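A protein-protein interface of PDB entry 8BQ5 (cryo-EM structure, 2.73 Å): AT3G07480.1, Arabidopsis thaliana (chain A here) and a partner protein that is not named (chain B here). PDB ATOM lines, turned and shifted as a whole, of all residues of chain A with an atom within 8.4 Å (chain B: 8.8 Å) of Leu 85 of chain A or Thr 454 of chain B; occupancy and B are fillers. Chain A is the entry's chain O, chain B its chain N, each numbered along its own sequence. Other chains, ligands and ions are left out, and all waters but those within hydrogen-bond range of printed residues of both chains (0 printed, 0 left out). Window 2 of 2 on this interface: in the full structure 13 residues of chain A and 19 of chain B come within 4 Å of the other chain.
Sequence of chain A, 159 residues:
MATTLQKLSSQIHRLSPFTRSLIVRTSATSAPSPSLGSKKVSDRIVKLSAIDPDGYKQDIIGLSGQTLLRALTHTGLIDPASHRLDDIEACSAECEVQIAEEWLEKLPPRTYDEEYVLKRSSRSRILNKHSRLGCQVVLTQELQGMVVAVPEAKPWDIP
The side-chain carboxylate (OD2) of Asp 87 of chain A lies within salt-bridge range of the guanidinium group (NH1) of Arg 446 of chain B, 3.9 Å away. The side-chain hydroxyl (OH) of Tyr 373 of chain B lies within hydrogen-bond range of the side-chain carboxylate (OE2) of Glu 94 of chain A.
The guanidinium group (NH1) of Arg 446 of chain B lies within salt-bridge range of the side-chain carboxylate (OD2) of Asp 450 of chain B, at 3.4 Å. The backbone carbonyl oxygen (O) of Asp 376 of chain B sits at hydrogen-bond distance from the side-chain hydroxyl (OH) of Tyr 458 of chain B (2.6 Å). The backbone NH of Tyr 373 of chain B sits at hydrogen-bond distance from the side-chain carboxylate of Asp 376 of chain B, 2.9 Å away. The side-chain carboxylate of Asp 87 of chain A lies within hydrogen-bond range of the backbone NH of Glu 89 of chain A (2.6 Å). A ring nitrogen (ND1) of His 83 of chain A is in hydrogen-bond range of the backbone carbonyl oxygen of Leu 85 of chain A, at 2.7 Å.
Arg 84 of chain A touches Thr 454 of chain B (O to CG2, 3.9 Å). Ala 375 of chain B touches Leu 85 of chain A. Asp 376 of chain B touches Leu 85 of chain A (OD1 to CD1, 3.7 Å). Leu 85 of chain A touches Thr 454 of chain B. Ile 456 of chain B touches Leu 85 of chain A. Asp 87 of chain A touches Ala 375 of chain B (OD2 to CB, 3.8 Å). Glu 89 of chain A touches Tyr 373 of chain B (O to CD1, 3.7 Å). Tyr 373 of chain B touches Ala 90 of chain A. Tyr 373 of chain B touches Cys 91 of chain A (OH to C, 3.7 Å).
Leu 85 of chain A touches just these residues of chain B: Ala 375, Asp 376, Thr 454 and Ile 456. No residue of chain B comes within 4 Å of Asp 86 of chain A. Printed residues of chain B within 4 Å of Glu 89 of chain A: Tyr 373. Of the printed residues of chain B, Cys 91 of chain A touches Tyr 373. Printed residues of chain A within 4 Å of Ala 375 of chain B: Leu 85 and Asp 87. Printed residues of chain A within 4 Å of Arg 446 of chain B: Asp 87 (3.9 Å). Printed residues of chain A within 4 Å of Thr 454 of chain B: Arg 84 and Leu 85. Of the printed residues of chain A, Ile 456 of chain B touches Leu 85 (3.8 Å). The nearest printed residue of chain B that does not touch Cys 91 of chain A is Ala 375 of chain B (7.2 Å).
Of the 18 printed residues of chain B, 6 touch a printed residue of chain A. Hydrophobic or aromatic side chains of chain B within 4 Å of the printed part of chain A: Tyr 373, Ala 375 and Ile 456. Hydrophobic or aromatic side chains of chain A that line the printed part of chain B: Leu 85 and Ala 90. Among the printed residues, Asp or Glu carboxylates within 4 Å of a Lys or Arg side-chain nitrogen of the other chain: Asp 87 of chain A with Arg 446 of chain B.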
ATOM      1  N   THR A  67      24.368  41.657   3.425  1.00  0.00           N
ATOM      2  CA  THR A  67      23.262  41.393   2.522  1.00  0.00           C
ATOM      3  C   THR A  67      21.925  41.469   3.252  1.00  0.00           C
ATOM      4  O   THR A  67      21.852  41.394   4.480  1.00  0.00           O
ATOM      5  CB  THR A  67      23.421  40.025   1.855  1.00  0.00           C
ATOM      6  OG1 THR A  67      23.339  38.991   2.842  1.00  0.00           O
ATOM      7  CG2 THR A  67      24.763  39.939   1.148  1.00  0.00           C
ATOM      8  N   LEU A  69      19.823  39.148   2.980  1.00  0.00           N
ATOM      9  CA  LEU A  69      19.612  37.787   3.461  1.00  0.00           C
ATOM     10  C   LEU A  69      20.073  37.635   4.905  1.00  0.00           C
ATOM     11  O   LEU A  69      19.404  36.978   5.706  1.00  0.00           O
ATOM     12  CB  LEU A  69      20.341  36.790   2.561  1.00  0.00           C
ATOM     13  CG  LEU A  69      20.493  35.372   3.119  1.00  0.00           C
ATOM     14  CD1 LEU A  69      19.139  34.696   3.280  1.00  0.00           C
ATOM     15  CD2 LEU A  69      21.413  34.536   2.252  1.00  0.00           C
ATOM     16  N   ARG A  70      21.218  38.224   5.253  1.00  0.00           N
ATOM     17  CA  ARG A  70      21.727  38.103   6.617  1.00  0.00           C
ATOM     18  C   ARG A  70      20.811  38.796   7.618  1.00  0.00           C
ATOM     19  O   ARG A  70      20.552  38.270   8.711  1.00  0.00           O
ATOM     20  CB  ARG A  70      23.140  38.676   6.696  1.00  0.00           C
ATOM     21  CG  ARG A  70      23.742  38.620   8.086  1.00  0.00           C
ATOM     22  CD  ARG A  70      24.263  37.230   8.397  1.00  0.00           C
ATOM     23  NE  ARG A  70      24.976  36.657   7.262  1.00  0.00           N
ATOM     24  CZ  ARG A  70      26.212  36.984   6.911  1.00  0.00           C
ATOM     25  NH1 ARG A  70      26.911  37.876   7.593  1.00  0.00           N
ATOM     26  NH2 ARG A  70      26.759  36.406   5.846  1.00  0.00           N
ATOM     27  N   PRO A  80      18.581  30.302   8.269  1.00  0.00           N
ATOM     28  CA  PRO A  80      19.999  30.405   7.888  1.00  0.00           C
ATOM     29  C   PRO A  80      20.557  29.129   7.288  1.00  0.00           C
ATOM     30  O   PRO A  80      21.435  29.198   6.421  1.00  0.00           O
ATOM     31  CB  PRO A  80      20.694  30.771   9.208  1.00  0.00           C
ATOM     32  CG  PRO A  80      19.719  30.435  10.282  1.00  0.00           C
ATOM     33  CD  PRO A  80      18.361  30.612   9.691  1.00  0.00           C
ATOM     34  N   ALA A  81      20.069  27.962   7.719  1.00  0.00           N
ATOM     35  CA  ALA A  81      20.556  26.700   7.171  1.00  0.00           C
ATOM     36  C   ALA A  81      20.226  26.540   5.695  1.00  0.00           C
ATOM     37  O   ALA A  81      20.951  25.839   4.980  1.00  0.00           O
ATOM     38  CB  ALA A  81      19.974  25.528   7.963  1.00  0.00           C
ATOM     39  N   SER A  82      19.153  27.170   5.219  1.00  0.00           N
ATOM     40  CA  SER A  82      18.754  27.037   3.825  1.00  0.00           C
ATOM     41  C   SER A  82      19.630  27.843   2.875  1.00  0.00           C
ATOM     42  O   SER A  82      19.592  27.601   1.664  1.00  0.00           O
ATOM     43  CB  SER A  82      17.299  27.469   3.659  1.00  0.00           C
ATOM     44  OG  SER A  82      17.205  28.877   3.554  1.00  0.00           O
ATOM     45  N   HIS A  83      20.391  28.807   3.389  1.00  0.00           N
ATOM     46  CA  HIS A  83      21.227  29.672   2.554  1.00  0.00           C
ATOM     47  C   HIS A  83      22.420  30.096   3.412  1.00  0.00           C
ATOM     48  O   HIS A  83      22.355  31.094   4.132  1.00  0.00           O
ATOM     49  CB  HIS A  83      20.430  30.870   2.060  1.00  0.00           C
ATOM     50  CG  HIS A  83      20.912  31.441   0.765  1.00  0.00           C
ATOM     51  ND1 HIS A  83      22.247  31.607   0.466  1.00  0.00           N
ATOM     52  CD2 HIS A  83      20.228  31.895  -0.309  1.00  0.00           C
ATOM     53  CE1 HIS A  83      22.362  32.138  -0.739  1.00  0.00           C
ATOM     54  NE2 HIS A  83      21.151  32.322  -1.230  1.00  0.00           N
ATOM     55  N   ARG A  84      23.507  29.335   3.320  1.00  0.00           N
ATOM     56  CA  ARG A  84      24.631  29.540   4.226  1.00  0.00           C
ATOM     57  C   ARG A  84      25.710  30.451   3.657  1.00  0.00           C
ATOM     58  O   ARG A  84      26.481  31.029   4.430  1.00  0.00           O
ATOM     59  CB  ARG A  84      25.246  28.192   4.612  1.00  0.00           C
ATOM     60  CG  ARG A  84      24.499  27.485   5.735  1.00  0.00           C
ATOM     61  CD  ARG A  84      25.131  26.148   6.074  1.00  0.00           C
ATOM     62  NE  ARG A  84      25.118  25.242   4.932  1.00  0.00           N
ATOM     63  CZ  ARG A  84      25.601  24.008   4.945  1.00  0.00           C
ATOM     64  NH1 ARG A  84      26.129  23.484   6.038  1.00  0.00           N
ATOM     65  NH2 ARG A  84      25.557  23.282   3.834  1.00  0.00           N
ATOM     66  N   LEU A  85      25.783  30.599   2.340  1.00  0.00           N
ATOM     67  CA  LEU A  85      26.741  31.483   1.698  1.00  0.00           C
ATOM     68  C   LEU A  85      26.002  32.617   1.001  1.00  0.00           C
ATOM     69  O   LEU A  85      24.842  32.480   0.614  1.00  0.00           O
ATOM     70  CB  LEU A  85      27.603  30.718   0.687  1.00  0.00           C
ATOM     71  CG  LEU A  85      28.249  29.406   1.136  1.00  0.00           C
ATOM     72  CD1 LEU A  85      29.193  28.899   0.060  1.00  0.00           C
ATOM     73  CD2 LEU A  85      28.981  29.566   2.459  1.00  0.00           C
ATOM     74  N   ASP A  86      26.690  33.744   0.831  1.00  0.00           N
ATOM     75  CA  ASP A  86      26.149  34.897   0.110  1.00  0.00           C
ATOM     76  C   ASP A  86      26.584  34.901  -1.347  1.00  0.00           C
ATOM     77  O   ASP A  86      26.857  35.956  -1.922  1.00  0.00           O
ATOM     78  CB  ASP A  86      26.557  36.204   0.786  1.00  0.00           C
ATOM     79  CG  ASP A  86      25.758  36.492   2.039  1.00  0.00           C
ATOM     80  OD1 ASP A  86      24.512  36.519   1.962  1.00  0.00           O
ATOM     81  OD2 ASP A  86      26.378  36.705   3.099  1.00  0.00           O
ATOM     82  N   ASP A  87      26.681  33.726  -1.958  1.00  0.00           N
ATOM     83  CA  ASP A  87      27.213  33.573  -3.303  1.00  0.00           C
ATOM     84  C   ASP A  87      26.079  33.230  -4.262  1.00  0.00           C
ATOM     85  O   ASP A  87      25.143  32.508  -3.904  1.00  0.00           O
ATOM     86  CB  ASP A  87      28.293  32.484  -3.313  1.00  0.00           C
ATOM     87  CG  ASP A  87      28.848  32.187  -4.698  1.00  0.00           C
ATOM     88  OD1 ASP A  87      28.390  32.759  -5.710  1.00  0.00           O
ATOM     89  OD2 ASP A  87      29.772  31.355  -4.766  1.00  0.00           O
ATOM     90  N   ILE A  88      26.168  33.764  -5.482  1.00  0.00           N
ATOM     91  CA  ILE A  88      25.166  33.473  -6.501  1.00  0.00           C
ATOM     92  C   ILE A  88      25.263  32.022  -6.957  1.00  0.00           C
ATOM     93  O   ILE A  88      24.283  31.450  -7.449  1.00  0.00           O
ATOM     94  CB  ILE A  88      25.307  34.459  -7.679  1.00  0.00           C
ATOM     95  CG1 ILE A  88      24.144  34.307  -8.655  1.00  0.00           C
ATOM     96  CG2 ILE A  88      26.629  34.261  -8.402  1.00  0.00           C
ATOM     97  CD1 ILE A  88      22.811  34.496  -8.014  1.00  0.00           C
ATOM     98  N   GLU A  89      26.432  31.397  -6.792  1.00  0.00           N
ATOM     99  CA  GLU A  89      26.612  30.006  -7.188  1.00  0.00           C
ATOM    100  C   GLU A  89      26.122  29.021  -6.136  1.00  0.00           C
ATOM    101  O   GLU A  89      26.134  27.813  -6.387  1.00  0.00           O
ATOM    102  CB  GLU A  89      28.082  29.737  -7.506  1.00  0.00           C
ATOM    103  CG  GLU A  89      28.733  30.826  -8.335  1.00  0.00           C
ATOM    104  CD  GLU A  89      28.696  30.518  -9.817  1.00  0.00           C
ATOM    105  OE1 GLU A  89      28.967  29.356 -10.192  1.00  0.00           O
ATOM    106  OE2 GLU A  89      28.381  31.432 -10.607  1.00  0.00           O
ATOM    107  N   ALA A  90      25.703  29.501  -4.972  1.00  0.00           N
ATOM    108  CA  ALA A  90      25.094  28.669  -3.944  1.00  0.00           C
ATOM    109  C   ALA A  90      23.689  29.164  -3.635  1.00  0.00           C
ATOM    110  O   ALA A  90      23.288  29.283  -2.475  1.00  0.00           O
ATOM    111  CB  ALA A  90      25.956  28.636  -2.686  1.00  0.00           C
ATOM    112  N   CYS A  91      22.929  29.468  -4.682  1.00  0.00           N
ATOM    113  CA  CYS A  91      21.605  30.057  -4.548  1.00  0.00           C
ATOM    114  C   CYS A  91      20.622  29.316  -5.441  1.00  0.00           C
ATOM    115  O   CYS A  91      20.881  29.129  -6.633  1.00  0.00           O
ATOM    116  CB  CYS A  91      21.633  31.545  -4.914  1.00  0.00           C
ATOM    117  SG  CYS A  91      20.019  32.346  -4.935  1.00  0.00           S
ATOM    118  N   GLU A  94      16.400  30.542  -2.533  1.00  0.00           N
ATOM    119  CA  GLU A  94      15.948  30.450  -1.151  1.00  0.00           C
ATOM    120  C   GLU A  94      15.881  31.821  -0.498  1.00  0.00           C
ATOM    121  O   GLU A  94      15.086  32.025   0.425  1.00  0.00           O
ATOM    122  CB  GLU A  94      16.878  29.545  -0.343  1.00  0.00           C
ATOM    123  CG  GLU A  94      16.988  28.124  -0.858  1.00  0.00           C
ATOM    124  CD  GLU A  94      18.148  27.938  -1.816  1.00  0.00           C
ATOM    125  OE1 GLU A  94      18.725  28.951  -2.268  1.00  0.00           O
ATOM    126  OE2 GLU A  94      18.493  26.775  -2.106  1.00  0.00           O
ATOM    127  N   CYS A  95      16.691  32.762  -0.970  1.00  0.00           N
ATOM    128  CA  CYS A  95      16.760  34.117  -0.447  1.00  0.00           C
ATOM    129  C   CYS A  95      15.806  35.074  -1.145  1.00  0.00           C
ATOM    130  O   CYS A  95      15.858  36.277  -0.875  1.00  0.00           O
ATOM    131  CB  CYS A  95      18.187  34.645  -0.578  1.00  0.00           C
ATOM    132  SG  CYS A  95      18.794  34.589  -2.272  1.00  0.00           S
ATOM    133  N   GLY A 134      17.843  37.917  -2.329  1.00  0.00           N
ATOM    134  CA  GLY A 134      18.282  38.592  -1.118  1.00  0.00           C
ATOM    135  C   GLY A 134      19.778  38.517  -0.889  1.00  0.00           C
ATOM    136  O   GLY A 134      20.356  39.398  -0.250  1.00  0.00           O
ATOM    137  N   CYS A 135      20.426  37.470  -1.404  1.00  0.00           N
ATOM    138  CA  CYS A 135      21.865  37.327  -1.231  1.00  0.00           C
ATOM    139  C   CYS A 135      22.657  38.303  -2.090  1.00  0.00           C
ATOM    140  O   CYS A 135      23.859  38.472  -1.864  1.00  0.00           O
ATOM    141  CB  CYS A 135      22.289  35.892  -1.547  1.00  0.00           C
ATOM    142  SG  CYS A 135      22.218  35.455  -3.296  1.00  0.00           S
ATOM    143  N   GLN A 136      22.019  38.944  -3.065  1.00  0.00           N
ATOM    144  CA  GLN A 136      22.683  39.903  -3.937  1.00  0.00           C
ATOM    145  C   GLN A 136      22.377  41.350  -3.579  1.00  0.00           C
ATOM    146  O   GLN A 136      23.005  42.255  -4.135  1.00  0.00           O
ATOM    147  CB  GLN A 136      22.296  39.643  -5.396  1.00  0.00           C
ATOM    148  CG  GLN A 136      22.599  38.237  -5.873  1.00  0.00           C
ATOM    149  CD  GLN A 136      24.077  37.917  -5.832  1.00  0.00           C
ATOM    150  OE1 GLN A 136      24.867  38.477  -6.592  1.00  0.00           O
ATOM    151  NE2 GLN A 136      24.462  37.009  -4.943  1.00  0.00           N
ATOM    152  N   TYR B 373      26.023  22.433  -2.827  1.00  0.00           N
ATOM    153  CA  TYR B 373      26.563  23.138  -3.978  1.00  0.00           C
ATOM    154  C   TYR B 373      28.057  22.877  -4.103  1.00  0.00           C
ATOM    155  O   TYR B 373      28.726  22.521  -3.129  1.00  0.00           O
ATOM    156  CB  TYR B 373      26.322  24.644  -3.872  1.00  0.00           C
ATOM    157  CG  TYR B 373      24.869  25.044  -3.790  1.00  0.00           C
ATOM    158  CD1 TYR B 373      24.087  25.118  -4.933  1.00  0.00           C
ATOM    159  CD2 TYR B 373      24.288  25.371  -2.573  1.00  0.00           C
ATOM    160  CE1 TYR B 373      22.761  25.490  -4.865  1.00  0.00           C
ATOM    161  CE2 TYR B 373      22.964  25.746  -2.496  1.00  0.00           C
ATOM    162  CZ  TYR B 373      22.205  25.803  -3.644  1.00  0.00           C
ATOM    163  OH  TYR B 373      20.886  26.177  -3.570  1.00  0.00           O
ATOM    164  N   ILE B 374      28.574  23.058  -5.318  1.00  0.00           N
ATOM    165  CA  ILE B 374      30.017  22.970  -5.528  1.00  0.00           C
ATOM    166  C   ILE B 374      30.728  24.061  -4.738  1.00  0.00           C
ATOM    167  O   ILE B 374      31.808  23.842  -4.178  1.00  0.00           O
ATOM    168  CB  ILE B 374      30.346  23.046  -7.030  1.00  0.00           C
ATOM    169  CG1 ILE B 374      29.908  21.764  -7.741  1.00  0.00           C
ATOM    170  CG2 ILE B 374      31.830  23.281  -7.248  1.00  0.00           C
ATOM    171  CD1 ILE B 374      29.507  21.985  -9.179  1.00  0.00           C
ATOM    172  N   ALA B 375      30.120  25.248  -4.664  1.00  0.00           N
ATOM    173  CA  ALA B 375      30.691  26.351  -3.903  1.00  0.00           C
ATOM    174  C   ALA B 375      30.827  26.031  -2.420  1.00  0.00           C
ATOM    175  O   ALA B 375      31.617  26.683  -1.729  1.00  0.00           O
ATOM    176  CB  ALA B 375      29.838  27.606  -4.086  1.00  0.00           C
ATOM    177  N   ASP B 376      30.077  25.049  -1.913  1.00  0.00           N
ATOM    178  CA  ASP B 376      30.200  24.664  -0.512  1.00  0.00           C
ATOM    179  C   ASP B 376      31.557  24.044  -0.205  1.00  0.00           C
ATOM    180  O   ASP B 376      31.923  23.930   0.970  1.00  0.00           O
ATOM    181  CB  ASP B 376      29.089  23.682  -0.132  1.00  0.00           C
ATOM    182  CG  ASP B 376      27.711  24.311  -0.172  1.00  0.00           C
ATOM    183  OD1 ASP B 376      27.615  25.555  -0.119  1.00  0.00           O
ATOM    184  OD2 ASP B 376      26.719  23.556  -0.253  1.00  0.00           O
ATOM    185  N   LEU B 377      32.314  23.665  -1.230  1.00  0.00           N
ATOM    186  CA  LEU B 377      33.634  23.026  -1.020  1.00  0.00           C
ATOM    187  C   LEU B 377      34.725  24.099  -0.863  1.00  0.00           C
ATOM    188  O   LEU B 377      35.898  23.714  -0.854  1.00  0.00           O
ATOM    189  CB  LEU B 377      33.933  22.117  -2.213  1.00  0.00           C
ATOM    190  CG  LEU B 377      32.855  21.101  -2.582  1.00  0.00           C
ATOM    191  CD1 LEU B 377      33.137  20.499  -3.949  1.00  0.00           C
ATOM    192  CD2 LEU B 377      32.762  20.012  -1.529  1.00  0.00           C
ATOM    193  N   GLY B 378      34.360  25.383  -0.777  1.00  0.00           N
ATOM    194  CA  GLY B 378      35.371  26.421  -0.675  1.00  0.00           C
ATOM    195  C   GLY B 378      36.228  26.251   0.567  1.00  0.00           C
ATOM    196  O   GLY B 378      35.740  25.892   1.641  1.00  0.00           O
ATOM    197  N   ALA B 379      37.528  26.505   0.405  1.00  0.00           N
ATOM    198  CA  ALA B 379      38.527  26.421   1.469  1.00  0.00           C
ATOM    199  C   ALA B 379      38.625  25.028   2.085  1.00  0.00           C
ATOM    200  O   ALA B 379      39.046  24.888   3.235  1.00  0.00           O
ATOM    201  CB  ALA B 379      38.262  27.458   2.566  1.00  0.00           C
ATOM    202  N   THR B 383      40.624  23.469   5.527  1.00  0.00           N
ATOM    203  CA  THR B 383      39.919  22.894   6.666  1.00  0.00           C
ATOM    204  C   THR B 383      40.074  21.384   6.761  1.00  0.00           C
ATOM    205  O   THR B 383      39.819  20.819   7.828  1.00  0.00           O
ATOM    206  CB  THR B 383      38.434  23.253   6.592  1.00  0.00           C
ATOM    207  OG1 THR B 383      37.838  22.608   5.461  1.00  0.00           O
ATOM    208  CG2 THR B 383      38.273  24.751   6.436  1.00  0.00           C
ATOM    209  N   ARG B 446      37.806  25.263  -6.896  1.00  0.00           N
ATOM    210  CA  ARG B 446      36.989  25.674  -5.758  1.00  0.00           C
ATOM    211  C   ARG B 446      37.634  25.263  -4.442  1.00  0.00           C
ATOM    212  O   ARG B 446      37.630  26.032  -3.474  1.00  0.00           O
ATOM    213  CB  ARG B 446      35.586  25.078  -5.869  1.00  0.00           C
ATOM    214  CG  ARG B 446      34.650  25.502  -4.749  1.00  0.00           C
ATOM    215  CD  ARG B 446      34.394  26.994  -4.778  1.00  0.00           C
ATOM    216  NE  ARG B 446      33.553  27.374  -5.905  1.00  0.00           N
ATOM    217  CZ  ARG B 446      32.967  28.555  -6.037  1.00  0.00           C
ATOM    218  NH1 ARG B 446      33.145  29.517  -5.145  1.00  0.00           N
ATOM    219  NH2 ARG B 446      32.187  28.779  -7.089  1.00  0.00           N
ATOM    220  N   ASP B 450      40.062  29.289  -4.396  1.00  0.00           N
ATOM    221  CA  ASP B 450      39.140  30.328  -3.968  1.00  0.00           C
ATOM    222  C   ASP B 450      39.370  30.702  -2.509  1.00  0.00           C
ATOM    223  O   ASP B 450      39.853  29.902  -1.703  1.00  0.00           O
ATOM    224  CB  ASP B 450      37.694  29.879  -4.171  1.00  0.00           C
ATOM    225  CG  ASP B 450      37.212  30.102  -5.588  1.00  0.00           C
ATOM    226  OD1 ASP B 450      37.629  31.105  -6.206  1.00  0.00           O
ATOM    227  OD2 ASP B 450      36.424  29.274  -6.087  1.00  0.00           O
ATOM    228  N   THR B 451      39.021  31.944  -2.179  1.00  0.00           N
ATOM    229  CA  THR B 451      39.145  32.482  -0.824  1.00  0.00           C
ATOM    230  C   THR B 451      37.806  33.099  -0.446  1.00  0.00           C
ATOM    231  O   THR B 451      37.644  34.327  -0.465  1.00  0.00           O
ATOM    232  CB  THR B 451      40.279  33.504  -0.729  1.00  0.00           C
ATOM    233  OG1 THR B 451      40.151  34.469  -1.780  1.00  0.00           O
ATOM    234  CG2 THR B 451      41.628  32.815  -0.842  1.00  0.00           C
ATOM    235  N   PRO B 452      36.821  32.275  -0.098  1.00  0.00           N
ATOM    236  CA  PRO B 452      35.484  32.800   0.194  1.00  0.00           C
ATOM    237  C   PRO B 452      35.446  33.563   1.509  1.00  0.00           C
ATOM    238  O   PRO B 452      36.251  33.346   2.416  1.00  0.00           O
ATOM    239  CB  PRO B 452      34.604  31.546   0.261  1.00  0.00           C
ATOM    240  CG  PRO B 452      35.532  30.373   0.273  1.00  0.00           C
ATOM    241  CD  PRO B 452      36.948  30.847   0.228  1.00  0.00           C
ATOM    242  N   ARG B 453      34.481  34.480   1.595  1.00  0.00           N
ATOM    243  CA  ARG B 453      34.270  35.218   2.836  1.00  0.00           C
ATOM    244  C   ARG B 453      33.755  34.307   3.945  1.00  0.00           C
ATOM    245  O   ARG B 453      34.170  34.434   5.101  1.00  0.00           O
ATOM    246  CB  ARG B 453      33.308  36.380   2.598  1.00  0.00           C
ATOM    247  CG  ARG B 453      32.857  37.092   3.863  1.00  0.00           C
ATOM    248  CD  ARG B 453      33.971  37.942   4.464  1.00  0.00           C
ATOM    249  NE  ARG B 453      33.676  38.451   5.802  1.00  0.00           N
ATOM    250  CZ  ARG B 453      33.268  37.729   6.840  1.00  0.00           C
ATOM    251  NH1 ARG B 453      33.169  36.411   6.780  1.00  0.00           N
ATOM    252  NH2 ARG B 453      32.974  38.347   7.981  1.00  0.00           N
ATOM    253  N   THR B 454      32.858  33.385   3.614  1.00  0.00           N
ATOM    254  CA  THR B 454      32.283  32.466   4.585  1.00  0.00           C
ATOM    255  C   THR B 454      32.704  31.044   4.247  1.00  0.00           C
ATOM    256  O   THR B 454      32.595  30.616   3.093  1.00  0.00           O
ATOM    257  CB  THR B 454      30.757  32.580   4.610  1.00  0.00           C
ATOM    258  OG1 THR B 454      30.384  33.861   5.130  1.00  0.00           O
ATOM    259  CG2 THR B 454      30.159  31.498   5.487  1.00  0.00           C
ATOM    260  N   TRP B 455      33.191  30.319   5.248  1.00  0.00           N
ATOM    261  CA  TRP B 455      33.615  28.938   5.087  1.00  0.00           C
ATOM    262  C   TRP B 455      32.557  27.997   5.649  1.00  0.00           C
ATOM    263  O   TRP B 455      31.693  28.398   6.430  1.00  0.00           O
ATOM    264  CB  TRP B 455      34.948  28.680   5.793  1.00  0.00           C
ATOM    265  CG  TRP B 455      36.126  29.420   5.229  1.00  0.00           C
ATOM    266  CD1 TRP B 455      36.105  30.444   4.330  1.00  0.00           C
ATOM    267  CD2 TRP B 455      37.504  29.195   5.548  1.00  0.00           C
ATOM    268  NE1 TRP B 455      37.384  30.866   4.063  1.00  0.00           N
ATOM    269  CE2 TRP B 455      38.261  30.116   4.801  1.00  0.00           C
ATOM    270  CE3 TRP B 455      38.170  28.304   6.395  1.00  0.00           C
ATOM    271  CZ2 TRP B 455      39.651  30.169   4.871  1.00  0.00           C
ATOM    272  CZ3 TRP B 455      39.547  28.358   6.462  1.00  0.00           C
ATOM    273  CH2 TRP B 455      40.274  29.284   5.706  1.00  0.00           C
ATOM    274  N   ILE B 456      32.634  26.737   5.238  1.00  0.00           N
ATOM    275  CA  ILE B 456      31.827  25.668   5.812  1.00  0.00           C
ATOM    276  C   ILE B 456      32.782  24.623   6.368  1.00  0.00           C
ATOM    277  O   ILE B 456      33.609  24.073   5.631  1.00  0.00           O
ATOM    278  CB  ILE B 456      30.866  25.058   4.783  1.00  0.00           C
ATOM    279  CG1 ILE B 456      29.722  26.027   4.487  1.00  0.00           C
ATOM    280  CG2 ILE B 456      30.308  23.747   5.297  1.00  0.00           C
ATOM    281  CD1 ILE B 456      29.102  25.836   3.130  1.00  0.00           C
ATOM    282  N   LEU B 457      32.674  24.358   7.665  1.00  0.00           N
ATOM    283  CA  LEU B 457      33.531  23.392   8.338  1.00  0.00           C
ATOM    284  C   LEU B 457      32.795  22.062   8.429  1.00  0.00           C
ATOM    285  O   LEU B 457      31.722  21.982   9.037  1.00  0.00           O
ATOM    286  CB  LEU B 457      33.922  23.892   9.728  1.00  0.00           C
ATOM    287  CG  LEU B 457      34.429  25.334   9.806  1.00  0.00           C
ATOM    288  CD1 LEU B 457      34.824  25.694  11.229  1.00  0.00           C
ATOM    289  CD2 LEU B 457      35.594  25.548   8.859  1.00  0.00           C
ATOM    290  N   TYR B 458      33.380  21.023   7.846  1.00  0.00           N
ATOM    291  CA  TYR B 458      32.722  19.733   7.696  1.00  0.00           C
ATOM    292  C   TYR B 458      33.109  18.786   8.825  1.00  0.00           C
ATOM    293  O   TYR B 458      34.267  18.745   9.250  1.00  0.00           O
ATOM    294  CB  TYR B 458      33.076  19.113   6.344  1.00  0.00           C
ATOM    295  CG  TYR B 458      32.453  19.850   5.185  1.00  0.00           C
ATOM    296  CD1 TYR B 458      31.179  19.529   4.741  1.00  0.00           C
ATOM    297  CD2 TYR B 458      33.123  20.887   4.555  1.00  0.00           C
ATOM    298  CE1 TYR B 458      30.597  20.206   3.693  1.00  0.00           C
ATOM    299  CE2 TYR B 458      32.549  21.571   3.505  1.00  0.00           C
ATOM    300  CZ  TYR B 458      31.287  21.225   3.078  1.00  0.00           C
ATOM    301  OH  TYR B 458      30.708  21.901   2.032  1.00  0.00           O
